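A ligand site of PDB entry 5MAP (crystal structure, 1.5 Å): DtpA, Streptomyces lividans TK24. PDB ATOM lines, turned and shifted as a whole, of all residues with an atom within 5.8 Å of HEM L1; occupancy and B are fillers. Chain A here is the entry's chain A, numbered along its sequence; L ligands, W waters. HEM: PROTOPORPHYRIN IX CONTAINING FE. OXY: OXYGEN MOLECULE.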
ATOM      1  N   ASN A 177      14.021  14.279  -7.304  1.00  0.00           N
ATOM      2  CA  ASN A 177      15.232  14.030  -8.080  1.00  0.00           C
ATOM      3  C   ASN A 177      14.883  13.886  -9.575  1.00  0.00           C
ATOM      4  O   ASN A 177      13.728  14.034 -10.041  1.00  0.00           O
ATOM      5  CB  ASN A 177      15.939  12.787  -7.548  1.00  0.00           C
ATOM      6  CG  ASN A 177      15.130  11.533  -7.701  1.00  0.00           C
ATOM      7  OD1 ASN A 177      14.394  11.391  -8.628  1.00  0.00           O
ATOM      8  ND2 ASN A 177      15.318  10.571  -6.769  1.00  0.00           N
ATOM      9  N   MET A 179      14.790  11.409 -11.484  1.00  0.00           N
ATOM     10  CA  MET A 179      13.907  10.280 -11.750  1.00  0.00           C
ATOM     11  C   MET A 179      12.410  10.610 -11.473  1.00  0.00           C
ATOM     12  O   MET A 179      11.530   9.792 -11.772  1.00  0.00           O
ATOM     13  CB  MET A 179      14.333   8.994 -11.035  1.00  0.00           C
ATOM     14  CG  MET A 179      15.509   8.270 -11.749  1.00  0.00           C
ATOM     15  SD  MET A 179      16.089   6.913 -10.695  1.00  0.00           S
ATOM     16  CE  MET A 179      16.961   5.938 -11.924  1.00  0.00           C
ATOM     17  N   GLN A 181      11.203  11.180  -8.482  1.00  0.00           N
ATOM     18  CA  GLN A 181      10.768  10.650  -7.189  1.00  0.00           C
ATOM     19  C   GLN A 181      10.860  11.724  -6.131  1.00  0.00           C
ATOM     20  O   GLN A 181      11.776  12.545  -6.096  1.00  0.00           O
ATOM     21  CB  GLN A 181      11.691   9.479  -6.775  1.00  0.00           C
ATOM     22  CG  GLN A 181      11.631   8.353  -7.806  1.00  0.00           C
ATOM     23  CD  GLN A 181      12.950   7.621  -8.024  1.00  0.00           C
ATOM     24  OE1 GLN A 181      14.000   8.016  -7.547  1.00  0.00           O
ATOM     25  NE2 GLN A 181      12.897   6.500  -8.733  1.00  0.00           N
ATOM     26  N   VAL A 182       9.956  11.622  -5.172  1.00  0.00           N
ATOM     27  CA  VAL A 182      10.071  12.359  -3.942  1.00  0.00           C
ATOM     28  C   VAL A 182      11.300  11.821  -3.221  1.00  0.00           C
ATOM     29  O   VAL A 182      11.406  10.633  -2.994  1.00  0.00           O
ATOM     30  CB  VAL A 182       8.781  12.167  -3.123  1.00  0.00           C
ATOM     31  CG1 VAL A 182       8.905  12.855  -1.770  1.00  0.00           C
ATOM     32  CG2 VAL A 182       7.548  12.715  -3.816  1.00  0.00           C
ATOM     33  N   ASP A 183      12.212  12.683  -2.855  1.00  0.00           N
ATOM     34  CA  ASP A 183      13.513  12.263  -2.389  1.00  0.00           C
ATOM     35  C   ASP A 183      13.910  13.022  -1.105  1.00  0.00           C
ATOM     36  O   ASP A 183      14.187  14.219  -1.146  1.00  0.00           O
ATOM     37  CB  ASP A 183      14.557  12.524  -3.513  1.00  0.00           C
ATOM     38  CG  ASP A 183      15.858  11.778  -3.311  1.00  0.00           C
ATOM     39  OD1 ASP A 183      16.144  11.460  -2.157  1.00  0.00           O
ATOM     40  OD2 ASP A 183      16.599  11.435  -4.293  1.00  0.00           O
ATOM     41  N   GLY A 184      13.860  12.304   0.025  1.00  0.00           N
ATOM     42  CA  GLY A 184      14.299  12.834   1.314  1.00  0.00           C
ATOM     43  C   GLY A 184      13.276  12.647   2.407  1.00  0.00           C
ATOM     44  O   GLY A 184      13.509  12.995   3.530  1.00  0.00           O
ATOM     45  N   THR A 185      12.161  11.999   2.130  1.00  0.00           N
ATOM     46  CA  THR A 185      11.142  11.779   3.132  1.00  0.00           C
ATOM     47  C   THR A 185      11.591  11.238   4.485  1.00  0.00           C
ATOM     48  O   THR A 185      11.260  11.842   5.551  1.00  0.00           O
ATOM     49  CB  THR A 185      10.077  10.855   2.590  1.00  0.00           C
ATOM     50  OG1 THR A 185       9.637  11.400   1.362  1.00  0.00           O
ATOM     51  CG2 THR A 185       8.937  10.646   3.585  1.00  0.00           C
ATOM     52  N   ARG A 186      12.316  10.142   4.436  1.00  0.00           N
ATOM     53  CA  ARG A 186      12.773   9.460   5.629  1.00  0.00           C
ATOM     54  C   ARG A 186      14.191   9.861   6.068  1.00  0.00           C
ATOM     55  O   ARG A 186      14.819   9.118   6.730  1.00  0.00           O
ATOM     56  CB  ARG A 186      12.655   7.954   5.464  1.00  0.00           C
ATOM     57  CG  ARG A 186      11.165   7.499   5.474  1.00  0.00           C
ATOM     58  CD  ARG A 186      10.743   6.739   6.727  1.00  0.00           C
ATOM     59  NE  ARG A 186      11.622   5.552   6.861  1.00  0.00           N
ATOM     60  CZ  ARG A 186      11.742   4.804   7.943  1.00  0.00           C
ATOM     61  NH1 ARG A 186      12.590   3.809   7.930  1.00  0.00           N
ATOM     62  NH2 ARG A 186      11.057   5.080   9.055  1.00  0.00           N
ATOM     63  N   ASN A 187      14.652  11.024   5.666  1.00  0.00           N
ATOM     64  CA  ASN A 187      15.962  11.566   6.166  1.00  0.00           C
ATOM     65  C   ASN A 187      15.777  11.880   7.621  1.00  0.00           C
ATOM     66  O   ASN A 187      14.875  12.679   7.944  1.00  0.00           O
ATOM     67  CB  ASN A 187      16.296  12.824   5.416  1.00  0.00           C
ATOM     68  CG  ASN A 187      17.700  13.368   5.702  1.00  0.00           C
ATOM     69  OD1 ASN A 187      18.640  12.612   5.891  1.00  0.00           O
ATOM     70  ND2 ASN A 187      17.843  14.694   5.650  1.00  0.00           N
ATOM     71  N   ARG A 224      28.825  10.029  -3.736  1.00  0.00           N
ATOM     72  CA  ARG A 224      28.790   9.165  -4.887  1.00  0.00           C
ATOM     73  C   ARG A 224      28.166   9.920  -6.058  1.00  0.00           C
ATOM     74  O   ARG A 224      27.017  10.446  -5.947  1.00  0.00           O
ATOM     75  CB  ARG A 224      27.966   7.902  -4.597  1.00  0.00           C
ATOM     76  CG  ARG A 224      28.419   7.184  -3.320  1.00  0.00           C
ATOM     77  CD  ARG A 224      29.726   6.415  -3.490  1.00  0.00           C
ATOM     78  NE  ARG A 224      29.477   5.209  -4.305  1.00  0.00           N
ATOM     79  CZ  ARG A 224      30.260   4.115  -4.397  1.00  0.00           C
ATOM     80  NH1 ARG A 224      31.462   4.095  -3.804  1.00  0.00           N
ATOM     81  NH2 ARG A 224      29.858   3.086  -5.154  1.00  0.00           N
ATOM     82  N   ILE A 226      26.259   9.441  -9.007  1.00  0.00           N
ATOM     83  CA  ILE A 226      25.475   8.325  -9.470  1.00  0.00           C
ATOM     84  C   ILE A 226      24.728   8.811 -10.676  1.00  0.00           C
ATOM     85  O   ILE A 226      23.777   9.597 -10.599  1.00  0.00           O
ATOM     86  CB  ILE A 226      24.493   7.806  -8.406  1.00  0.00           C
ATOM     87  CG1 ILE A 226      25.173   7.631  -7.027  1.00  0.00           C
ATOM     88  CG2 ILE A 226      23.869   6.543  -8.905  1.00  0.00           C
ATOM     89  CD1 ILE A 226      24.236   7.105  -5.974  1.00  0.00           C
ATOM     90  N   ARG A 227      25.127   8.328 -11.846  1.00  0.00           N
ATOM     91  CA  ARG A 227      24.379   8.628 -13.057  1.00  0.00           C
ATOM     92  C   ARG A 227      23.074   7.901 -13.117  1.00  0.00           C
ATOM     93  O   ARG A 227      22.971   6.749 -12.731  1.00  0.00           O
ATOM     94  CB  ARG A 227      25.276   8.257 -14.271  1.00  0.00           C
ATOM     95  CG  ARG A 227      24.635   8.586 -15.591  1.00  0.00           C
ATOM     96  CD  ARG A 227      25.615   8.806 -16.704  1.00  0.00           C
ATOM     97  NE  ARG A 227      26.207   7.524 -17.065  1.00  0.00           N
ATOM     98  CZ  ARG A 227      25.666   6.631 -17.875  1.00  0.00           C
ATOM     99  NH1 ARG A 227      26.305   5.486 -18.144  1.00  0.00           N
ATOM    100  NH2 ARG A 227      24.540   6.860 -18.459  1.00  0.00           N
ATOM    101  N   MET A 228      22.035   8.583 -13.562  1.00  0.00           N
ATOM    102  CA  MET A 228      20.767   7.955 -13.681  1.00  0.00           C
ATOM    103  C   MET A 228      20.628   7.568 -15.150  1.00  0.00           C
ATOM    104  O   MET A 228      20.811   8.368 -16.003  1.00  0.00           O
ATOM    105  CB  MET A 228      19.647   8.906 -13.220  1.00  0.00           C
ATOM    106  CG  MET A 228      19.557   9.138 -11.757  1.00  0.00           C
ATOM    107  SD  MET A 228      18.469  10.537 -11.492  1.00  0.00           S
ATOM    108  CE  MET A 228      18.016  10.154  -9.790  1.00  0.00           C
ATOM    109  N   ILE A 245      11.001   1.562  -6.431  1.00  0.00           N
ATOM    110  CA  ILE A 245      11.259   2.311  -5.139  1.00  0.00           C
ATOM    111  C   ILE A 245      10.424   1.773  -3.970  1.00  0.00           C
ATOM    112  O   ILE A 245      10.916   1.701  -2.866  1.00  0.00           O
ATOM    113  CB  ILE A 245      11.052   3.822  -5.286  1.00  0.00           C
ATOM    114  CG1 ILE A 245      11.996   4.328  -6.396  1.00  0.00           C
ATOM    115  CG2 ILE A 245      11.245   4.555  -3.921  1.00  0.00           C
ATOM    116  CD1 ILE A 245      13.400   4.437  -5.968  1.00  0.00           C
ATOM    117  N   ARG A 247       7.581   3.301  -3.289  1.00  0.00           N
ATOM    118  CA  ARG A 247       6.733   4.443  -2.975  1.00  0.00           C
ATOM    119  C   ARG A 247       6.171   5.049  -4.250  1.00  0.00           C
ATOM    120  O   ARG A 247       6.755   4.963  -5.302  1.00  0.00           O
ATOM    121  CB  ARG A 247       7.482   5.511  -2.239  1.00  0.00           C
ATOM    122  CG  ARG A 247       8.020   5.115  -0.872  1.00  0.00           C
ATOM    123  CD  ARG A 247       9.062   6.073  -0.294  1.00  0.00           C
ATOM    124  NE  ARG A 247       9.304   5.786   1.114  1.00  0.00           N
ATOM    125  CZ  ARG A 247       8.461   6.009   2.142  1.00  0.00           C
ATOM    126  NH1 ARG A 247       7.346   6.743   2.033  1.00  0.00           N
ATOM    127  NH2 ARG A 247       8.838   5.566   3.347  1.00  0.00           N
ATOM    128  N   HIS A 285      13.672  -0.292  -3.423  1.00  0.00           N
ATOM    129  CA  HIS A 285      14.730   0.472  -2.788  1.00  0.00           C
ATOM    130  C   HIS A 285      14.405   1.013  -1.406  1.00  0.00           C
ATOM    131  O   HIS A 285      15.265   0.989  -0.484  1.00  0.00           O
ATOM    132  CB  HIS A 285      15.042   1.642  -3.741  1.00  0.00           C
ATOM    133  CG  HIS A 285      16.138   2.554  -3.269  1.00  0.00           C
ATOM    134  ND1 HIS A 285      17.483   2.282  -3.456  1.00  0.00           N
ATOM    135  CD2 HIS A 285      16.091   3.765  -2.675  1.00  0.00           C
ATOM    136  CE1 HIS A 285      18.200   3.269  -2.947  1.00  0.00           C
ATOM    137  NE2 HIS A 285      17.361   4.165  -2.481  1.00  0.00           N
ATOM    138  N   ALA A 286      13.215   1.568  -1.238  1.00  0.00           N
ATOM    139  CA  ALA A 286      12.817   2.159   0.054  1.00  0.00           C
ATOM    140  C   ALA A 286      12.434   1.103   1.093  1.00  0.00           C
ATOM    141  O   ALA A 286      12.038   1.487   2.206  1.00  0.00           O
ATOM    142  CB  ALA A 286      11.698   3.202  -0.141  1.00  0.00           C
ATOM    143  N   THR A 289      16.705  -0.361   1.958  1.00  0.00           N
ATOM    144  CA  THR A 289      17.595   0.616   2.512  1.00  0.00           C
ATOM    145  C   THR A 289      17.277   1.040   3.979  1.00  0.00           C
ATOM    146  O   THR A 289      18.082   1.732   4.604  1.00  0.00           O
ATOM    147  CB  THR A 289      17.576   1.907   1.688  1.00  0.00           C
ATOM    148  OG1 THR A 289      16.266   2.335   1.606  1.00  0.00           O
ATOM    149  CG2 THR A 289      18.208   1.772   0.341  1.00  0.00           C
ATOM    150  N   ARG A 290      16.117   0.637   4.540  1.00  0.00           N
ATOM    151  CA  ARG A 290      15.718   1.102   5.869  1.00  0.00           C
ATOM    152  C   ARG A 290      16.680   0.627   6.961  1.00  0.00           C
ATOM    153  O   ARG A 290      17.218  -0.494   6.886  1.00  0.00           O
ATOM    154  CB  ARG A 290      14.329   0.642   6.235  1.00  0.00           C
ATOM    155  CG  ARG A 290      13.239   1.084   5.290  1.00  0.00           C
ATOM    156  CD  ARG A 290      11.997   0.211   5.396  1.00  0.00           C
ATOM    157  NE  ARG A 290      11.443   0.180   6.754  1.00  0.00           N
ATOM    158  CZ  ARG A 290      10.497   1.007   7.197  1.00  0.00           C
ATOM    159  NH1 ARG A 290      10.040   1.996   6.475  1.00  0.00           N
ATOM    160  NH2 ARG A 290      10.042   0.861   8.426  1.00  0.00           N
ATOM    161  N   PRO A 291      16.936   1.490   7.953  1.00  0.00           N
ATOM    162  CA  PRO A 291      17.637   1.048   9.166  1.00  0.00           C
ATOM    163  C   PRO A 291      17.138  -0.297   9.705  1.00  0.00           C
ATOM    164  O   PRO A 291      17.951  -1.170   9.918  1.00  0.00           O
ATOM    165  CB  PRO A 291      17.432   2.237  10.142  1.00  0.00           C
ATOM    166  CG  PRO A 291      17.351   3.418   9.258  1.00  0.00           C
ATOM    167  CD  PRO A 291      16.543   2.915   8.081  1.00  0.00           C
ATOM    168  N   MET A 299      21.847   6.817   8.007  1.00  0.00           N
ATOM    169  CA  MET A 299      22.559   7.921   7.430  1.00  0.00           C
ATOM    170  C   MET A 299      21.585   9.051   7.210  1.00  0.00           C
ATOM    171  O   MET A 299      20.427   8.808   6.940  1.00  0.00           O
ATOM    172  CB  MET A 299      23.234   7.529   6.102  1.00  0.00           C
ATOM    173  CG  MET A 299      22.276   7.246   4.958  1.00  0.00           C
ATOM    174  SD  MET A 299      23.059   6.188   3.727  1.00  0.00           S
ATOM    175  CE  MET A 299      22.652   4.703   4.611  1.00  0.00           C
ATOM    176  N   ARG A 301      20.898  11.759   4.361  1.00  0.00           N
ATOM    177  CA  ARG A 301      21.091  11.989   2.940  1.00  0.00           C
ATOM    178  C   ARG A 301      20.788  13.404   2.591  1.00  0.00           C
ATOM    179  O   ARG A 301      19.700  13.909   2.942  1.00  0.00           O
ATOM    180  CB  ARG A 301      20.182  11.091   2.168  1.00  0.00           C
ATOM    181  CG  ARG A 301      20.556   9.633   2.255  1.00  0.00           C
ATOM    182  CD  ARG A 301      19.479   8.661   1.796  1.00  0.00           C
ATOM    183  NE  ARG A 301      18.226   8.791   2.557  1.00  0.00           N
ATOM    184  CZ  ARG A 301      17.038   9.091   2.058  1.00  0.00           C
ATOM    185  NH1 ARG A 301      16.863   9.269   0.731  1.00  0.00           N
ATOM    186  NH2 ARG A 301      15.970   9.183   2.896  1.00  0.00           N
ATOM    187  N   LEU A 320      22.279  11.876  -9.684  1.00  0.00           N
ATOM    188  CA  LEU A 320      22.361  12.328  -8.299  1.00  0.00           C
ATOM    189  C   LEU A 320      23.779  12.394  -7.772  1.00  0.00           C
ATOM    190  O   LEU A 320      24.554  11.424  -7.892  1.00  0.00           O
ATOM    191  CB  LEU A 320      21.579  11.344  -7.413  1.00  0.00           C
ATOM    192  CG  LEU A 320      21.159  11.840  -6.018  1.00  0.00           C
ATOM    193  CD1 LEU A 320      20.090  12.900  -6.060  1.00  0.00           C
ATOM    194  CD2 LEU A 320      20.563  10.641  -5.294  1.00  0.00           C
ATOM    195  N   PHE A 322      24.851  12.038  -4.752  1.00  0.00           N
ATOM    196  CA  PHE A 322      24.515  11.468  -3.429  1.00  0.00           C
ATOM    197  C   PHE A 322      25.539  11.811  -2.385  1.00  0.00           C
ATOM    198  O   PHE A 322      26.690  11.584  -2.628  1.00  0.00           O
ATOM    199  CB  PHE A 322      24.500   9.974  -3.644  1.00  0.00           C
ATOM    200  CG  PHE A 322      24.183   9.164  -2.454  1.00  0.00           C
ATOM    201  CD1 PHE A 322      22.913   8.925  -2.115  1.00  0.00           C
ATOM    202  CD2 PHE A 322      25.221   8.706  -1.645  1.00  0.00           C
ATOM    203  CE1 PHE A 322      22.594   8.119  -1.001  1.00  0.00           C
ATOM    204  CE2 PHE A 322      24.926   7.926  -0.523  1.00  0.00           C
ATOM    205  CZ  PHE A 322      23.594   7.656  -0.227  1.00  0.00           C
ATOM    206  N   PHE A 333      26.460   4.001   5.155  1.00  0.00           N
ATOM    207  CA  PHE A 333      26.653   3.715   3.723  1.00  0.00           C
ATOM    208  C   PHE A 333      27.089   2.293   3.366  1.00  0.00           C
ATOM    209  O   PHE A 333      26.485   1.648   2.471  1.00  0.00           O
ATOM    210  CB  PHE A 333      27.633   4.680   3.073  1.00  0.00           C
ATOM    211  CG  PHE A 333      27.841   4.420   1.612  1.00  0.00           C
ATOM    212  CD1 PHE A 333      26.991   4.988   0.707  1.00  0.00           C
ATOM    213  CD2 PHE A 333      28.888   3.676   1.143  1.00  0.00           C
ATOM    214  CE1 PHE A 333      27.156   4.773  -0.629  1.00  0.00           C
ATOM    215  CE2 PHE A 333      29.054   3.452  -0.203  1.00  0.00           C
ATOM    216  CZ  PHE A 333      28.207   3.999  -1.101  1.00  0.00           C
ATOM    217  N   VAL A 336      24.638  -0.759   3.762  1.00  0.00           N
ATOM    218  CA  VAL A 336      23.433  -0.528   2.908  1.00  0.00           C
ATOM    219  C   VAL A 336      23.807  -0.745   1.440  1.00  0.00           C
ATOM    220  O   VAL A 336      23.180  -1.523   0.714  1.00  0.00           O
ATOM    221  CB  VAL A 336      22.726   0.830   3.146  1.00  0.00           C
ATOM    222  CG1 VAL A 336      21.657   1.109   2.116  1.00  0.00           C
ATOM    223  CG2 VAL A 336      22.088   0.941   4.557  1.00  0.00           C
ATOM    224  N   GLN A 337      24.896  -0.115   1.011  1.00  0.00           N
ATOM    225  CA  GLN A 337      25.349  -0.309  -0.352  1.00  0.00           C
ATOM    226  C   GLN A 337      25.762  -1.757  -0.716  1.00  0.00           C
ATOM    227  O   GLN A 337      25.502  -2.200  -1.837  1.00  0.00           O
ATOM    228  CB  GLN A 337      26.454   0.722  -0.648  1.00  0.00           C
ATOM    229  CG  GLN A 337      26.955   0.755  -2.120  1.00  0.00           C
ATOM    230  CD  GLN A 337      25.869   0.957  -3.153  1.00  0.00           C
ATOM    231  OE1 GLN A 337      24.842   1.559  -2.841  1.00  0.00           O
ATOM    232  NE2 GLN A 337      26.127   0.549  -4.373  1.00  0.00           N
ATOM    233  N   LEU A 340      22.584  -3.101  -1.521  1.00  0.00           N
ATOM    234  CA  LEU A 340      21.970  -2.530  -2.724  1.00  0.00           C
ATOM    235  C   LEU A 340      22.604  -3.026  -4.016  1.00  0.00           C
ATOM    236  O   LEU A 340      21.934  -3.214  -5.030  1.00  0.00           O
ATOM    237  CB  LEU A 340      21.986  -1.010  -2.722  1.00  0.00           C
ATOM    238  CG  LEU A 340      21.319  -0.230  -1.624  1.00  0.00           C
ATOM    239  CD1 LEU A 340      21.254   1.221  -2.080  1.00  0.00           C
ATOM    240  CD2 LEU A 340      19.984  -0.793  -1.272  1.00  0.00           C
ATOM    241  N   LEU A 346      16.637  -0.796  -7.996  1.00  0.00           N
ATOM    242  CA  LEU A 346      17.163   0.443  -8.610  1.00  0.00           C
ATOM    243  C   LEU A 346      18.432   0.289  -9.314  1.00  0.00           C
ATOM    244  O   LEU A 346      18.753   1.125 -10.143  1.00  0.00           O
ATOM    245  CB  LEU A 346      17.317   1.550  -7.557  1.00  0.00           C
ATOM    246  CG  LEU A 346      17.670   2.974  -7.977  1.00  0.00           C
ATOM    247  CD1 LEU A 346      16.612   3.601  -8.842  1.00  0.00           C
ATOM    248  CD2 LEU A 346      17.978   3.765  -6.697  1.00  0.00           C
ATOM    249  N   ILE A 350      20.902   2.824 -12.492  1.00  0.00           N
ATOM    250  CA  ILE A 350      21.884   3.772 -12.046  1.00  0.00           C
ATOM    251  C   ILE A 350      23.272   3.239 -12.302  1.00  0.00           C
ATOM    252  O   ILE A 350      23.484   2.040 -12.433  1.00  0.00           O
ATOM    253  CB  ILE A 350      21.680   4.126 -10.580  1.00  0.00           C
ATOM    254  CG1 ILE A 350      21.796   2.924  -9.613  1.00  0.00           C
ATOM    255  CG2 ILE A 350      20.334   4.773 -10.396  1.00  0.00           C
ATOM    256  CD1 ILE A 350      22.100   3.308  -8.142  1.00  0.00           C
ATOM    257  N   HIS A 352      27.100   4.088 -10.417  1.00  0.00           N
ATOM    258  CA  HIS A 352      27.986   4.826  -9.626  1.00  0.00           C
ATOM    259  C   HIS A 352      29.324   5.119 -10.350  1.00  0.00           C
ATOM    260  O   HIS A 352      30.059   4.172 -10.700  1.00  0.00           O
ATOM    261  CB  HIS A 352      28.290   4.053  -8.367  1.00  0.00           C
ATOM    262  CG  HIS A 352      27.147   3.930  -7.414  1.00  0.00           C
ATOM    263  ND1 HIS A 352      27.176   4.436  -6.157  1.00  0.00           N
ATOM    264  CD2 HIS A 352      25.931   3.315  -7.533  1.00  0.00           C
ATOM    265  CE1 HIS A 352      26.063   4.117  -5.508  1.00  0.00           C
ATOM    266  NE2 HIS A 352      25.284   3.434  -6.328  1.00  0.00           N
HETATM  267  CHA HEM L   1      15.307   6.355   0.293  1.00  0.00           C
HETATM  268  CHB HEM L   1      16.114   7.381  -4.361  1.00  0.00           C
HETATM  269  CHC HEM L   1      20.761   5.997  -3.930  1.00  0.00           C
HETATM  270  CHD HEM L   1      19.950   5.104   0.808  1.00  0.00           C
HETATM  271  C1A HEM L   1      15.151   6.767  -1.012  1.00  0.00           C
HETATM  272  C2A HEM L   1      13.901   7.171  -1.580  1.00  0.00           C
HETATM  273  C3A HEM L   1      14.150   7.478  -2.886  1.00  0.00           C
HETATM  274  C4A HEM L   1      15.524   7.195  -3.127  1.00  0.00           C
HETATM  275  CMA HEM L   1      13.142   7.950  -3.915  1.00  0.00           C
HETATM  276  CAA HEM L   1      12.580   7.247  -0.843  1.00  0.00           C
HETATM  277  CBA HEM L   1      12.218   8.573  -0.223  1.00  0.00           C
HETATM  278  CGA HEM L   1      13.094   8.917   0.940  1.00  0.00           C
HETATM  279  O1A HEM L   1      12.948   8.397   2.060  1.00  0.00           O
HETATM  280  O2A HEM L   1      14.040   9.684   0.702  1.00  0.00           O
HETATM  281  C1B HEM L   1      17.478   7.100  -4.668  1.00  0.00           C
HETATM  282  C2B HEM L   1      18.120   7.310  -5.937  1.00  0.00           C
HETATM  283  C3B HEM L   1      19.405   6.919  -5.850  1.00  0.00           C
HETATM  284  C4B HEM L   1      19.570   6.486  -4.437  1.00  0.00           C
HETATM  285  CMB HEM L   1      17.454   7.779  -7.171  1.00  0.00           C
HETATM  286  CAB HEM L   1      20.540   6.950  -6.775  1.00  0.00           C
HETATM  287  CBB HEM L   1      20.524   7.631  -7.925  1.00  0.00           C
HETATM  288  C1C HEM L   1      20.952   5.565  -2.590  1.00  0.00           C
HETATM  289  C2C HEM L   1      22.151   5.051  -2.062  1.00  0.00           C
HETATM  290  C3C HEM L   1      21.905   4.792  -0.694  1.00  0.00           C
HETATM  291  C4C HEM L   1      20.552   5.200  -0.436  1.00  0.00           C
HETATM  292  CMC HEM L   1      23.421   4.849  -2.892  1.00  0.00           C
HETATM  293  CAC HEM L   1      22.794   4.188   0.343  1.00  0.00           C
HETATM  294  CBC HEM L   1      23.742   3.345   0.012  1.00  0.00           C
HETATM  295  C1D HEM L   1      18.650   5.429   1.028  1.00  0.00           C
HETATM  296  C2D HEM L   1      18.055   5.349   2.377  1.00  0.00           C
HETATM  297  C3D HEM L   1      16.725   5.688   2.211  1.00  0.00           C
HETATM  298  C4D HEM L   1      16.556   5.947   0.774  1.00  0.00           C
HETATM  299  CMD HEM L   1      18.748   4.954   3.680  1.00  0.00           C
HETATM  300  CAD HEM L   1      15.706   5.783   3.331  1.00  0.00           C
HETATM  301  CBD HEM L   1      15.155   4.422   3.734  1.00  0.00           C
HETATM  302  CGD HEM L   1      14.114   4.579   4.812  1.00  0.00           C
HETATM  303  O1D HEM L   1      12.866   4.702   4.497  1.00  0.00           O
HETATM  304  O2D HEM L   1      14.582   4.503   6.018  1.00  0.00           O
HETATM  305  NA  HEM L   1      16.114   6.753  -1.983  1.00  0.00           N
HETATM  306  NB  HEM L   1      18.373   6.633  -3.786  1.00  0.00           N
HETATM  307  NC  HEM L   1      19.963   5.574  -1.634  1.00  0.00           N
HETATM  308  ND  HEM L   1      17.700   5.736   0.090  1.00  0.00           N
HETATM  309 FE   HEM L   1      18.016   6.154  -1.811  1.00  0.00          FE
HETATM  310  O1  OXY L   2      18.302   8.433  -1.486  1.00  0.00           O
HETATM  311  O2  OXY L   2      18.326   9.590  -2.054  1.00  0.00           O
HETATM  312  O   HOH W   1       9.775   8.605  -2.650  1.00  0.00           O
HETATM  313  O   HOH W   2      16.135   6.290   7.183  1.00  0.00           O
HETATM  314  O   HOH W   3      10.791   3.241   3.968  1.00  0.00           O
HETATM  315  O   HOH W   4      11.908   5.914   2.267  1.00  0.00           O
HETATM  316  O   HOH W   5      19.575   3.163   6.352  1.00  0.00           O
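NE of Arg 186 is in salt-bridge range of O1D of HEM L1. NH1 of Arg 301 is in salt-bridge range of O2A of HEM L1, at 2.9 Å. The guanidinium group (NH1) of Arg 301 sits at hydrogen-bond distance from an oxygen (O2) of OXY L2 (3.2 Å). FE of HEM L1 is bound by NE2 of His 285. N of Thr 185 is in hydrogen-bond range of O2A of HEM L1 (3.3 Å). N of Gly 184 sits at hydrogen-bond distance from O2A of HEM L1, 2.7 Å away. N of Arg 186 sits at hydrogen-bond distance from O1A of HEM L1 (3.0 Å).
FE of HEM L1 is bound by O1 of OXY L2 (2.3 Å).
NE of Arg 224 sits at hydrogen-bond distance from ND1 of His 352. O of His 285 lies within hydrogen-bond range of OG1 of Thr 289, at 2.7 Å. The side-chain amide oxygen (OE1) of Gln 181 is in hydrogen-bond range of the side-chain amide nitrogen (ND2) of Asn 177 (3.0 Å). ND2 of Asn 177 sits at hydrogen-bond distance from OD2 of Asp 183, 2.9 Å away. The backbone NH (N) of Ile 226 sits at hydrogen-bond distance from the backbone carbonyl oxygen (O) of Leu 320, at 2.8 Å. N of His 285 lies within hydrogen-bond range of O of Ile 245 (3.4 Å). NE2 of Gln 181 sits close to SD of Met 179 (3.8 Å). The guanidinium group (NH1) of Arg 301 lies within salt-bridge range of the side-chain carboxylate (OD1) of Asp 183, 3.7 Å away.
Merely in contact with HEM L1: Asn 177, Met 179, Gln 181, Val 182, Asp 183, Ile 226, Met 228, Ile 245, Arg 247, Thr 289, Arg 290, Pro 291, Met 299, Leu 320, Phe 322, Phe 333, Val 336, Gln 337, Leu 340, Leu 346, Ile 350 and His 352. Hydrophobic or aromatic side chains within 4 Å of HEM L1: Met 179, Ile 226, Met 228, Ile 245, His 285, Pro 291, Met 299, Leu 320, Phe 322, Phe 333, Val 336, Leu 340, Leu 346, Ile 350 and His 352. The nearest printed residue that does not touch HEM L1 is Ala 286 (4.03 Å).
Water W3 lies within hydrogen-bond range of an oxygen (O1D) of HEM L1 (2.6 Å), the backbone carbonyl oxygen (O) of Ala 286 (2.8 Å), the guanidinium group (NH1) of Arg 290 (2.9 Å) and the guanidinium group (NH2) of Arg 247 (3.1 Å). Water W2 bridges an oxygen (O2D) of HEM L1 (2.6 Å) and the backbone carbonyl oxygen of Arg 186 (3.2 Å). Water W4 lies within hydrogen-bond range of an oxygen (O1A) of HEM L1 (2.7 Å) and the guanidinium group of Arg 247 (2.9 Å).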
